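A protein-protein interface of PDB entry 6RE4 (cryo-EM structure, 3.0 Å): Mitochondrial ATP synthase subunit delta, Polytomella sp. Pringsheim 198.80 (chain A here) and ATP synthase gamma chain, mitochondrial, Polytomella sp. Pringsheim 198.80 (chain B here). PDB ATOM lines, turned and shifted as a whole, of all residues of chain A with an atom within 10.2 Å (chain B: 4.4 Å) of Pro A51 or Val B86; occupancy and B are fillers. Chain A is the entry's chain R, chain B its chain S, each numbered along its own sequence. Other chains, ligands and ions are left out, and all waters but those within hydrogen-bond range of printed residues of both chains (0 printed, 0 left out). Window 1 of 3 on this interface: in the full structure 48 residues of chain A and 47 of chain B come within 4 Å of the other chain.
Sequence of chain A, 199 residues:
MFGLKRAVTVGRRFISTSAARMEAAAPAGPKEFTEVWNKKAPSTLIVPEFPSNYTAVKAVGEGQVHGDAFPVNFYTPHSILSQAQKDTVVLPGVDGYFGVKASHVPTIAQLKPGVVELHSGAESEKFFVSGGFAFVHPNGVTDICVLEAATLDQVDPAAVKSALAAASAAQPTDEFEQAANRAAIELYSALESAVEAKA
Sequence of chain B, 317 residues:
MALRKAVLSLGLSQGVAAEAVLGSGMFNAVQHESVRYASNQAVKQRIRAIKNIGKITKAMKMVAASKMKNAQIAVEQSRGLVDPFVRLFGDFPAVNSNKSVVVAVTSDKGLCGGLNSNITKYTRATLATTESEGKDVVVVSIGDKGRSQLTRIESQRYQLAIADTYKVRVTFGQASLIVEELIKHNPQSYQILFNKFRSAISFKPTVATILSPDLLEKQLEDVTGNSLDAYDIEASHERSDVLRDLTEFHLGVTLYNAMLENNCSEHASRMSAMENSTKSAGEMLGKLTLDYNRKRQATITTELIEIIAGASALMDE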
ATOM      1  N   GLY A  29      -5.503  11.235  30.790  1.00  0.00           N
ATOM      2  CA  GLY A  29      -6.222  11.130  29.549  1.00  0.00           C
ATOM      3  C   GLY A  29      -5.402  11.524  28.345  1.00  0.00           C
ATOM      4  O   GLY A  29      -4.331  12.122  28.460  1.00  0.00           O
ATOM      5  N   PRO A  30      -5.916  11.202  27.155  1.00  0.00           N
ATOM      6  CA  PRO A  30      -5.176  11.527  25.928  1.00  0.00           C
ATOM      7  C   PRO A  30      -5.115  13.012  25.649  1.00  0.00           C
ATOM      8  O   PRO A  30      -4.201  13.471  24.953  1.00  0.00           O
ATOM      9  CB  PRO A  30      -5.966  10.780  24.853  1.00  0.00           C
ATOM     10  CG  PRO A  30      -7.330  10.679  25.392  1.00  0.00           C
ATOM     11  CD  PRO A  30      -7.190  10.528  26.871  1.00  0.00           C
ATOM     12  N   PHE A  33      -2.228  13.714  28.431  1.00  0.00           N
ATOM     13  CA  PHE A  33      -0.947  13.077  28.143  1.00  0.00           C
ATOM     14  C   PHE A  33      -0.171  13.834  27.084  1.00  0.00           C
ATOM     15  O   PHE A  33       1.064  13.838  27.130  1.00  0.00           O
ATOM     16  CB  PHE A  33      -1.166  11.637  27.677  1.00  0.00           C
ATOM     17  CG  PHE A  33       0.102  10.883  27.398  1.00  0.00           C
ATOM     18  CD1 PHE A  33       0.536  10.685  26.097  1.00  0.00           C
ATOM     19  CD2 PHE A  33       0.846  10.355  28.433  1.00  0.00           C
ATOM     20  CE1 PHE A  33       1.690   9.990  25.843  1.00  0.00           C
ATOM     21  CE2 PHE A  33       1.997   9.649  28.185  1.00  0.00           C
ATOM     22  CZ  PHE A  33       2.420   9.470  26.888  1.00  0.00           C
ATOM     23  N   PRO A  48       1.877  10.084  20.396  1.00  0.00           N
ATOM     24  CA  PRO A  48       1.448   8.771  19.909  1.00  0.00           C
ATOM     25  C   PRO A  48      -0.046   8.601  20.029  1.00  0.00           C
ATOM     26  O   PRO A  48      -0.694   9.231  20.860  1.00  0.00           O
ATOM     27  CB  PRO A  48       2.180   7.793  20.828  1.00  0.00           C
ATOM     28  CG  PRO A  48       2.461   8.566  22.045  1.00  0.00           C
ATOM     29  CD  PRO A  48       2.741   9.953  21.580  1.00  0.00           C
ATOM     30  N   GLU A  49      -0.597   7.758  19.175  1.00  0.00           N
ATOM     31  CA  GLU A  49      -2.033   7.589  19.210  1.00  0.00           C
ATOM     32  C   GLU A  49      -2.441   6.681  20.363  1.00  0.00           C
ATOM     33  O   GLU A  49      -1.614   6.067  21.040  1.00  0.00           O
ATOM     34  CB  GLU A  49      -2.534   7.048  17.885  1.00  0.00           C
ATOM     35  CG  GLU A  49      -2.620   8.101  16.819  1.00  0.00           C
ATOM     36  CD  GLU A  49      -3.742   7.850  15.835  1.00  0.00           C
ATOM     37  OE1 GLU A  49      -4.888   7.634  16.280  1.00  0.00           O
ATOM     38  OE2 GLU A  49      -3.479   7.871  14.615  1.00  0.00           O
ATOM     39  N   PHE A  50      -3.744   6.628  20.598  1.00  0.00           N
ATOM     40  CA  PHE A  50      -4.356   5.943  21.718  1.00  0.00           C
ATOM     41  C   PHE A  50      -5.559   5.180  21.198  1.00  0.00           C
ATOM     42  O   PHE A  50      -6.166   5.599  20.212  1.00  0.00           O
ATOM     43  CB  PHE A  50      -4.805   6.936  22.797  1.00  0.00           C
ATOM     44  CG  PHE A  50      -3.811   8.020  23.084  1.00  0.00           C
ATOM     45  CD1 PHE A  50      -3.902   9.246  22.452  1.00  0.00           C
ATOM     46  CD2 PHE A  50      -2.794   7.815  23.992  1.00  0.00           C
ATOM     47  CE1 PHE A  50      -2.999  10.244  22.725  1.00  0.00           C
ATOM     48  CE2 PHE A  50      -1.879   8.812  24.261  1.00  0.00           C
ATOM     49  CZ  PHE A  50      -1.983  10.025  23.630  1.00  0.00           C
ATOM     50  N   PRO A  51      -5.927   4.060  21.828  1.00  0.00           N
ATOM     51  CA  PRO A  51      -7.076   3.286  21.339  1.00  0.00           C
ATOM     52  C   PRO A  51      -8.411   4.007  21.426  1.00  0.00           C
ATOM     53  O   PRO A  51      -9.334   3.627  20.700  1.00  0.00           O
ATOM     54  CB  PRO A  51      -7.064   2.042  22.233  1.00  0.00           C
ATOM     55  CG  PRO A  51      -6.211   2.396  23.387  1.00  0.00           C
ATOM     56  CD  PRO A  51      -5.193   3.323  22.867  1.00  0.00           C
ATOM     57  N   SER A  52      -8.535   5.052  22.247  1.00  0.00           N
ATOM     58  CA  SER A  52      -9.768   5.829  22.277  1.00  0.00           C
ATOM     59  C   SER A  52      -9.953   6.685  21.034  1.00  0.00           C
ATOM     60  O   SER A  52     -11.068   7.150  20.779  1.00  0.00           O
ATOM     61  CB  SER A  52      -9.807   6.726  23.509  1.00  0.00           C
ATOM     62  OG  SER A  52      -8.797   7.711  23.453  1.00  0.00           O
ATOM     63  N   ASN A  53      -8.891   6.912  20.263  1.00  0.00           N
ATOM     64  CA  ASN A  53      -9.001   7.664  19.024  1.00  0.00           C
ATOM     65  C   ASN A  53      -9.608   6.854  17.894  1.00  0.00           C
ATOM     66  O   ASN A  53      -9.981   7.432  16.869  1.00  0.00           O
ATOM     67  CB  ASN A  53      -7.629   8.173  18.593  1.00  0.00           C
ATOM     68  CG  ASN A  53      -6.864   8.794  19.725  1.00  0.00           C
ATOM     69  OD1 ASN A  53      -5.701   8.478  19.941  1.00  0.00           O
ATOM     70  ND2 ASN A  53      -7.510   9.683  20.465  1.00  0.00           N
ATOM     71  N   TYR A  54      -9.719   5.540  18.050  1.00  0.00           N
ATOM     72  CA  TYR A  54     -10.208   4.671  16.996  1.00  0.00           C
ATOM     73  C   TYR A  54     -11.623   4.192  17.230  1.00  0.00           C
ATOM     74  O   TYR A  54     -12.184   3.512  16.367  1.00  0.00           O
ATOM     75  CB  TYR A  54      -9.298   3.465  16.848  1.00  0.00           C
ATOM     76  CG  TYR A  54      -7.861   3.822  16.662  1.00  0.00           C
ATOM     77  CD1 TYR A  54      -7.407   4.305  15.450  1.00  0.00           C
ATOM     78  CD2 TYR A  54      -6.956   3.663  17.689  1.00  0.00           C
ATOM     79  CE1 TYR A  54      -6.092   4.626  15.273  1.00  0.00           C
ATOM     80  CE2 TYR A  54      -5.641   3.980  17.522  1.00  0.00           C
ATOM     81  CZ  TYR A  54      -5.218   4.466  16.318  1.00  0.00           C
ATOM     82  OH  TYR A  54      -3.901   4.763  16.143  1.00  0.00           O
ATOM     83  N   THR A  55     -12.215   4.519  18.369  1.00  0.00           N
ATOM     84  CA  THR A  55     -13.575   4.111  18.669  1.00  0.00           C
ATOM     85  C   THR A  55     -14.474   5.332  18.582  1.00  0.00           C
ATOM     86  O   THR A  55     -14.093   6.428  19.006  1.00  0.00           O
ATOM     87  CB  THR A  55     -13.669   3.433  20.041  1.00  0.00           C
ATOM     88  OG1 THR A  55     -15.036   3.134  20.337  1.00  0.00           O
ATOM     89  CG2 THR A  55     -13.067   4.284  21.147  1.00  0.00           C
ATOM     90  N   ALA A  56     -15.635   5.159  17.969  1.00  0.00           N
ATOM     91  CA  ALA A  56     -16.575   6.257  17.867  1.00  0.00           C
ATOM     92  C   ALA A  56     -17.636   6.220  18.946  1.00  0.00           C
ATOM     93  O   ALA A  56     -18.180   7.272  19.298  1.00  0.00           O
ATOM     94  CB  ALA A  56     -17.251   6.249  16.494  1.00  0.00           C
ATOM     95  N   VAL A  57     -17.913   5.050  19.504  1.00  0.00           N
ATOM     96  CA  VAL A  57     -19.050   4.852  20.388  1.00  0.00           C
ATOM     97  C   VAL A  57     -18.523   4.765  21.807  1.00  0.00           C
ATOM     98  O   VAL A  57     -17.716   3.885  22.129  1.00  0.00           O
ATOM     99  CB  VAL A  57     -19.841   3.596  20.015  1.00  0.00           C
ATOM    100  CG1 VAL A  57     -21.001   3.418  20.968  1.00  0.00           C
ATOM    101  CG2 VAL A  57     -20.314   3.682  18.578  1.00  0.00           C
ATOM    102  N   LYS A  58     -18.980   5.672  22.656  1.00  0.00           N
ATOM    103  CA  LYS A  58     -18.634   5.694  24.065  1.00  0.00           C
ATOM    104  C   LYS A  58     -19.780   5.095  24.874  1.00  0.00           C
ATOM    105  O   LYS A  58     -20.726   4.527  24.323  1.00  0.00           O
ATOM    106  CB  LYS A  58     -18.294   7.118  24.491  1.00  0.00           C
ATOM    107  CG  LYS A  58     -17.123   7.697  23.732  1.00  0.00           C
ATOM    108  CD  LYS A  58     -15.894   6.814  23.881  1.00  0.00           C
ATOM    109  CE  LYS A  58     -14.762   7.276  22.991  1.00  0.00           C
ATOM    110  NZ  LYS A  58     -15.036   7.062  21.548  1.00  0.00           N
ATOM    111  N   ALA A  59     -19.698   5.208  26.197  1.00  0.00           N
ATOM    112  CA  ALA A  59     -20.657   4.556  27.077  1.00  0.00           C
ATOM    113  C   ALA A  59     -21.614   5.503  27.777  1.00  0.00           C
ATOM    114  O   ALA A  59     -22.782   5.157  27.946  1.00  0.00           O
ATOM    115  CB  ALA A  59     -19.923   3.738  28.143  1.00  0.00           C
ATOM    116  N   VAL A  60     -21.159   6.672  28.214  1.00  0.00           N
ATOM    117  CA  VAL A  60     -22.024   7.542  29.000  1.00  0.00           C
ATOM    118  C   VAL A  60     -22.722   8.570  28.111  1.00  0.00           C
ATOM    119  O   VAL A  60     -23.625   9.279  28.580  1.00  0.00           O
ATOM    120  CB  VAL A  60     -21.201   8.202  30.126  1.00  0.00           C
ATOM    121  CG1 VAL A  60     -22.082   8.662  31.294  1.00  0.00           C
ATOM    122  CG2 VAL A  60     -20.128   7.252  30.630  1.00  0.00           C
ATOM    123  N   TYR A  75     -18.476 -10.015  20.079  1.00  0.00           N
ATOM    124  CA  TYR A  75     -17.045 -10.020  19.839  1.00  0.00           C
ATOM    125  C   TYR A  75     -16.412 -11.306  20.334  1.00  0.00           C
ATOM    126  O   TYR A  75     -16.791 -11.842  21.374  1.00  0.00           O
ATOM    127  CB  TYR A  75     -16.370  -8.855  20.532  1.00  0.00           C
ATOM    128  CG  TYR A  75     -16.677  -7.521  19.934  1.00  0.00           C
ATOM    129  CD1 TYR A  75     -16.755  -7.354  18.572  1.00  0.00           C
ATOM    130  CD2 TYR A  75     -16.882  -6.423  20.739  1.00  0.00           C
ATOM    131  CE1 TYR A  75     -17.044  -6.131  18.023  1.00  0.00           C
ATOM    132  CE2 TYR A  75     -17.165  -5.194  20.201  1.00  0.00           C
ATOM    133  CZ  TYR A  75     -17.246  -5.052  18.843  1.00  0.00           C
ATOM    134  OH  TYR A  75     -17.533  -3.819  18.317  1.00  0.00           O
ATOM    135  N   PHE A 135     -21.277  -6.389  28.622  1.00  0.00           N
ATOM    136  CA  PHE A 135     -21.541  -5.106  29.259  1.00  0.00           C
ATOM    137  C   PHE A 135     -22.726  -4.447  28.585  1.00  0.00           C
ATOM    138  O   PHE A 135     -22.875  -4.536  27.368  1.00  0.00           O
ATOM    139  CB  PHE A 135     -20.348  -4.159  29.159  1.00  0.00           C
ATOM    140  CG  PHE A 135     -19.034  -4.836  29.214  1.00  0.00           C
ATOM    141  CD1 PHE A 135     -18.615  -5.476  30.348  1.00  0.00           C
ATOM    142  CD2 PHE A 135     -18.195  -4.796  28.123  1.00  0.00           C
ATOM    143  CE1 PHE A 135     -17.399  -6.094  30.382  1.00  0.00           C
ATOM    144  CE2 PHE A 135     -16.980  -5.405  28.158  1.00  0.00           C
ATOM    145  CZ  PHE A 135     -16.578  -6.052  29.288  1.00  0.00           C
ATOM    146  N   HIS A 137     -24.243  -0.547  28.467  1.00  0.00           N
ATOM    147  CA  HIS A 137     -23.728   0.771  28.763  1.00  0.00           C
ATOM    148  C   HIS A 137     -24.866   1.761  28.944  1.00  0.00           C
ATOM    149  O   HIS A 137     -25.985   1.512  28.488  1.00  0.00           O
ATOM    150  CB  HIS A 137     -22.791   1.205  27.631  1.00  0.00           C
ATOM    151  CG  HIS A 137     -21.469   0.517  27.673  1.00  0.00           C
ATOM    152  ND1 HIS A 137     -20.894  -0.065  26.568  1.00  0.00           N
ATOM    153  CD2 HIS A 137     -20.627   0.282  28.703  1.00  0.00           C
ATOM    154  CE1 HIS A 137     -19.741  -0.607  26.913  1.00  0.00           C
ATOM    155  NE2 HIS A 137     -19.558  -0.415  28.205  1.00  0.00           N
ATOM    156  N   ASP A 143     -22.407  -4.867  24.729  1.00  0.00           N
ATOM    157  CA  ASP A 143     -21.147  -5.414  24.243  1.00  0.00           C
ATOM    158  C   ASP A 143     -20.974  -6.826  24.770  1.00  0.00           C
ATOM    159  O   ASP A 143     -20.520  -6.994  25.898  1.00  0.00           O
ATOM    160  CB  ASP A 143     -19.981  -4.560  24.702  1.00  0.00           C
ATOM    161  CG  ASP A 143     -19.800  -3.341  23.874  1.00  0.00           C
ATOM    162  OD1 ASP A 143     -19.963  -3.434  22.653  1.00  0.00           O
ATOM    163  OD2 ASP A 143     -19.466  -2.286  24.421  1.00  0.00           O
ATOM    164  N   CYS A 145     -18.762 -10.000  24.901  1.00  0.00           N
ATOM    165  CA  CYS A 145     -17.327 -10.197  24.724  1.00  0.00           C
ATOM    166  C   CYS A 145     -16.976 -11.591  25.215  1.00  0.00           C
ATOM    167  O   CYS A 145     -16.669 -11.773  26.390  1.00  0.00           O
ATOM    168  CB  CYS A 145     -16.565  -9.157  25.493  1.00  0.00           C
ATOM    169  SG  CYS A 145     -17.054  -7.493  25.120  1.00  0.00           S
ATOM    170  N   VAL B  82     -11.295  -4.715  21.247  1.00  0.00           N
ATOM    171  CA  VAL B  82     -10.609  -3.725  22.064  1.00  0.00           C
ATOM    172  C   VAL B  82     -11.522  -2.544  22.393  1.00  0.00           C
ATOM    173  O   VAL B  82     -11.308  -1.868  23.403  1.00  0.00           O
ATOM    174  CB  VAL B  82      -9.306  -3.306  21.351  1.00  0.00           C
ATOM    175  CG1 VAL B  82      -9.597  -2.566  20.068  1.00  0.00           C
ATOM    176  CG2 VAL B  82      -8.370  -2.521  22.265  1.00  0.00           C
ATOM    177  N   ASP B  83     -12.581  -2.327  21.619  1.00  0.00           N
ATOM    178  CA  ASP B  83     -13.483  -1.189  21.792  1.00  0.00           C
ATOM    179  C   ASP B  83     -14.357  -1.210  23.053  1.00  0.00           C
ATOM    180  O   ASP B  83     -14.507  -0.144  23.667  1.00  0.00           O
ATOM    181  CB  ASP B  83     -14.371  -1.030  20.556  1.00  0.00           C
ATOM    182  CG  ASP B  83     -13.591  -0.691  19.322  1.00  0.00           C
ATOM    183  OD1 ASP B  83     -13.897  -1.271  18.259  1.00  0.00           O
ATOM    184  OD2 ASP B  83     -12.679   0.156  19.408  1.00  0.00           O
ATOM    185  N   PRO B  84     -14.981  -2.333  23.474  1.00  0.00           N
ATOM    186  CA  PRO B  84     -15.767  -2.287  24.718  1.00  0.00           C
ATOM    187  C   PRO B  84     -14.967  -1.996  25.962  1.00  0.00           C
ATOM    188  O   PRO B  84     -15.513  -1.409  26.899  1.00  0.00           O
ATOM    189  CB  PRO B  84     -16.383  -3.685  24.794  1.00  0.00           C
ATOM    190  CG  PRO B  84     -15.588  -4.482  23.917  1.00  0.00           C
ATOM    191  CD  PRO B  84     -15.277  -3.608  22.799  1.00  0.00           C
ATOM    192  N   PHE B  85     -13.693  -2.346  25.996  1.00  0.00           N
ATOM    193  CA  PHE B  85     -12.893  -2.021  27.162  1.00  0.00           C
ATOM    194  C   PHE B  85     -12.495  -0.561  27.178  1.00  0.00           C
ATOM    195  O   PHE B  85     -12.420   0.051  28.246  1.00  0.00           O
ATOM    196  CB  PHE B  85     -11.665  -2.899  27.189  1.00  0.00           C
ATOM    197  CG  PHE B  85     -11.972  -4.313  27.445  1.00  0.00           C
ATOM    198  CD1 PHE B  85     -12.377  -4.713  28.697  1.00  0.00           C
ATOM    199  CD2 PHE B  85     -11.884  -5.243  26.440  1.00  0.00           C
ATOM    200  CE1 PHE B  85     -12.669  -6.012  28.938  1.00  0.00           C
ATOM    201  CE2 PHE B  85     -12.181  -6.542  26.685  1.00  0.00           C
ATOM    202  CZ  PHE B  85     -12.571  -6.922  27.932  1.00  0.00           C
ATOM    203  N   VAL B  86     -12.232   0.021  26.008  1.00  0.00           N
ATOM    204  CA  VAL B  86     -11.866   1.431  25.978  1.00  0.00           C
ATOM    205  C   VAL B  86     -13.075   2.340  26.004  1.00  0.00           C
ATOM    206  O   VAL B  86     -12.904   3.561  26.099  1.00  0.00           O
ATOM    207  CB  VAL B  86     -10.990   1.771  24.758  1.00  0.00           C
ATOM    208  CG1 VAL B  86      -9.803   0.833  24.687  1.00  0.00           C
ATOM    209  CG2 VAL B  86     -11.794   1.703  23.501  1.00  0.00           C
ATOM    210  N   ARG B  87     -14.293   1.802  25.929  1.00  0.00           N
ATOM    211  CA  ARG B  87     -15.437   2.615  26.317  1.00  0.00           C
ATOM    212  C   ARG B  87     -15.952   2.300  27.709  1.00  0.00           C
ATOM    213  O   ARG B  87     -16.671   3.121  28.280  1.00  0.00           O
ATOM    214  CB  ARG B  87     -16.588   2.499  25.314  1.00  0.00           C
ATOM    215  CG  ARG B  87     -17.161   1.137  25.081  1.00  0.00           C
ATOM    216  CD  ARG B  87     -18.385   1.285  24.210  1.00  0.00           C
ATOM    217  NE  ARG B  87     -18.754   0.069  23.506  1.00  0.00           N
ATOM    218  CZ  ARG B  87     -18.398  -0.187  22.256  1.00  0.00           C
ATOM    219  NH1 ARG B  87     -17.675   0.690  21.589  1.00  0.00           N
ATOM    220  NH2 ARG B  87     -18.777  -1.304  21.665  1.00  0.00           N
ATOM    221  N   LEU B  88     -15.586   1.158  28.280  1.00  0.00           N
ATOM    222  CA  LEU B  88     -15.967   0.842  29.647  1.00  0.00           C
ATOM    223  C   LEU B  88     -14.949   1.346  30.657  1.00  0.00           C
ATOM    224  O   LEU B  88     -15.330   1.915  31.681  1.00  0.00           O
ATOM    225  CB  LEU B  88     -16.166  -0.665  29.794  1.00  0.00           C
ATOM    226  CG  LEU B  88     -16.108  -1.290  31.183  1.00  0.00           C
ATOM    227  CD1 LEU B  88     -17.318  -0.919  31.982  1.00  0.00           C
ATOM    228  CD2 LEU B  88     -16.037  -2.783  31.051  1.00  0.00           C
ATOM    229  N   GLY B  90     -12.413   3.515  29.781  1.00  0.00           N
ATOM    230  CA  GLY B  90     -11.793   4.749  29.362  1.00  0.00           C
ATOM    231  C   GLY B  90     -10.413   4.513  28.775  1.00  0.00           C
ATOM    232  O   GLY B  90     -10.035   3.403  28.409  1.00  0.00           O
ATOM    233  N   ASP B  91      -9.645   5.598  28.707  1.00  0.00           N
ATOM    234  CA  ASP B  91      -8.285   5.546  28.179  1.00  0.00           C
ATOM    235  C   ASP B  91      -7.472   6.572  28.955  1.00  0.00           C
ATOM    236  O   ASP B  91      -7.539   7.764  28.656  1.00  0.00           O
ATOM    237  CB  ASP B  91      -8.265   5.843  26.691  1.00  0.00           C
ATOM    238  CG  ASP B  91      -7.159   5.123  25.969  1.00  0.00           C
ATOM    239  OD1 ASP B  91      -6.438   4.325  26.601  1.00  0.00           O
ATOM    240  OD2 ASP B  91      -7.020   5.355  24.754  1.00  0.00           O
ATOM    241  N   THR B 206       0.843   3.474  18.341  1.00  0.00           N
ATOM    242  CA  THR B 206      -0.204   3.628  19.335  1.00  0.00           C
ATOM    243  C   THR B 206       0.318   3.187  20.693  1.00  0.00           C
ATOM    244  O   THR B 206       0.962   2.141  20.798  1.00  0.00           O
ATOM    245  CB  THR B 206      -1.418   2.793  18.939  1.00  0.00           C
ATOM    246  OG1 THR B 206      -1.949   3.287  17.707  1.00  0.00           O
ATOM    247  CG2 THR B 206      -2.494   2.847  19.985  1.00  0.00           C
ATOM    248  N   VAL B 207       0.067   3.990  21.724  1.00  0.00           N
ATOM    249  CA  VAL B 207       0.303   3.573  23.099  1.00  0.00           C
ATOM    250  C   VAL B 207      -1.037   3.207  23.731  1.00  0.00           C
ATOM    251  O   VAL B 207      -2.044   3.893  23.527  1.00  0.00           O
ATOM    252  CB  VAL B 207       1.084   4.637  23.897  1.00  0.00           C
ATOM    253  CG1 VAL B 207       0.314   5.918  24.104  1.00  0.00           C
ATOM    254  CG2 VAL B 207       1.525   4.075  25.232  1.00  0.00           C
ATOM    255  N   ALA B 208      -1.076   2.062  24.407  1.00  0.00           N
ATOM    256  CA  ALA B 208      -2.300   1.509  24.964  1.00  0.00           C
ATOM    257  C   ALA B 208      -2.098   1.231  26.441  1.00  0.00           C
ATOM    258  O   ALA B 208      -1.097   0.621  26.824  1.00  0.00           O
ATOM    259  CB  ALA B 208      -2.699   0.228  24.239  1.00  0.00           C
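N of Pro A51 sits close to OD2 of Asp B91. O of Glu A49 lies within hydrogen-bond range of N of Val B207 (2.8 Å). The side-chain hydroxyl (OG1) of Thr B206 is in hydrogen-bond range of the side-chain hydroxyl (OH) of Tyr A54 (2.9 Å). The backbone carbonyl oxygen of Val A57 is in hydrogen-bond range of the guanidinium group of Arg B87 (3.2 Å). OD2 of Asp A143 is in salt-bridge range of NE of Arg B87 (2.6 Å). The backbone NH (N) of Ser A52 lies within hydrogen-bond range of the side-chain carboxylate (OD2) of Asp B91 (2.9 Å).
The backbone carbonyl oxygen of Phe A135 sits at hydrogen-bond distance from the backbone NH of Asp A143. The backbone NH (N) of Phe A50 sits at hydrogen-bond distance from the side-chain amide oxygen (OD1) of Asn A53. The side-chain amino group of Lys A58 sits at hydrogen-bond distance from the backbone carbonyl oxygen of Thr A55 (2.8 Å). OE1 of Glu A49 sits at hydrogen-bond distance from OH of Tyr A54. The side-chain sulfur of Cys A145 sits at hydrogen-bond distance from the backbone carbonyl oxygen of Asp A143, 3.6 Å away. ND1 of His A137 lies close to OD2 of Asp A143 (3.4 Å).
Gly A29 touches Asp B91 (CA to O, 3.7 Å). CG of Pro A48 touches CG1 of Val B207, at 3.98 Å. Phe A50 touches Val B207 (CA to O, 3.6 Å). Thr B206 touches Pro A51. Pro A51 touches Val B207. CG2 of Val B86 touches CG2 of Thr A55, at 3.7 Å. Thr A55 touches Arg B87. CD of Pro B84 touches CE2 of Tyr A75 (3.6 Å). Phe A135 touches Phe B85 (CZ to CE1, 3.9 Å). Asp A143 touches Pro B84.
Printed residues of chain B within 4 Å of Pro A51: Val B86, Asp B91, Thr B206 and Val B207. Val B86 touches just these residues of chain A: Pro A51 and Thr A55. Pro B84 touches just these residues of chain A: Tyr A75, Phe A135, Asp A143 and Cys A145. No residue of chain A comes within 4 Å of Gly B90. Printed residues of chain B within 4 Å of Tyr A54: Thr B206 (2.9 Å). Of the printed residues of chain B, Pro A48 touches Val B207. Of the printed residues of chain A, Arg B87 touches Thr A55 (3.8 Å), Val A57 (3.2 Å), Lys A58 (3.99 Å), Ala A59 (3.3 Å), His A137 (3.6 Å) and Asp A143 (2.6 Å). Printed residues of chain A within 4 Å of Val B207: Pro A48, Glu A49, Phe A50 and Pro A51. Ala A56 touches none of the printed residues of chain B. Ala B208 touches none of the printed residues of chain A.
Of the 21 printed residues of chain A, 17 touch a printed residue of chain B. Hydrophobic or aromatic side chains of chain A that line the printed part of chain B: Pro A30, Pro A48, Phe A50, Pro A51, Tyr A54, Val A57, Ala A59, Tyr A75, Phe A135 and His A137. Along chain A the printed residues that touch a printed residue of chain B span positions 29 to 145. Of the 12 printed residues of chain B, 9 touch a printed residue of chain A. Hydrophobic or aromatic side chains of chain B within 4 Å of the printed part of chain A: Pro B84, Phe B85, Val B86, Leu B88 and Val B207. Among the printed residues, Asp or Glu carboxylates within 4 Å of a Lys or Arg side-chain nitrogen of the other chain: Asp A143 with Arg B87.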
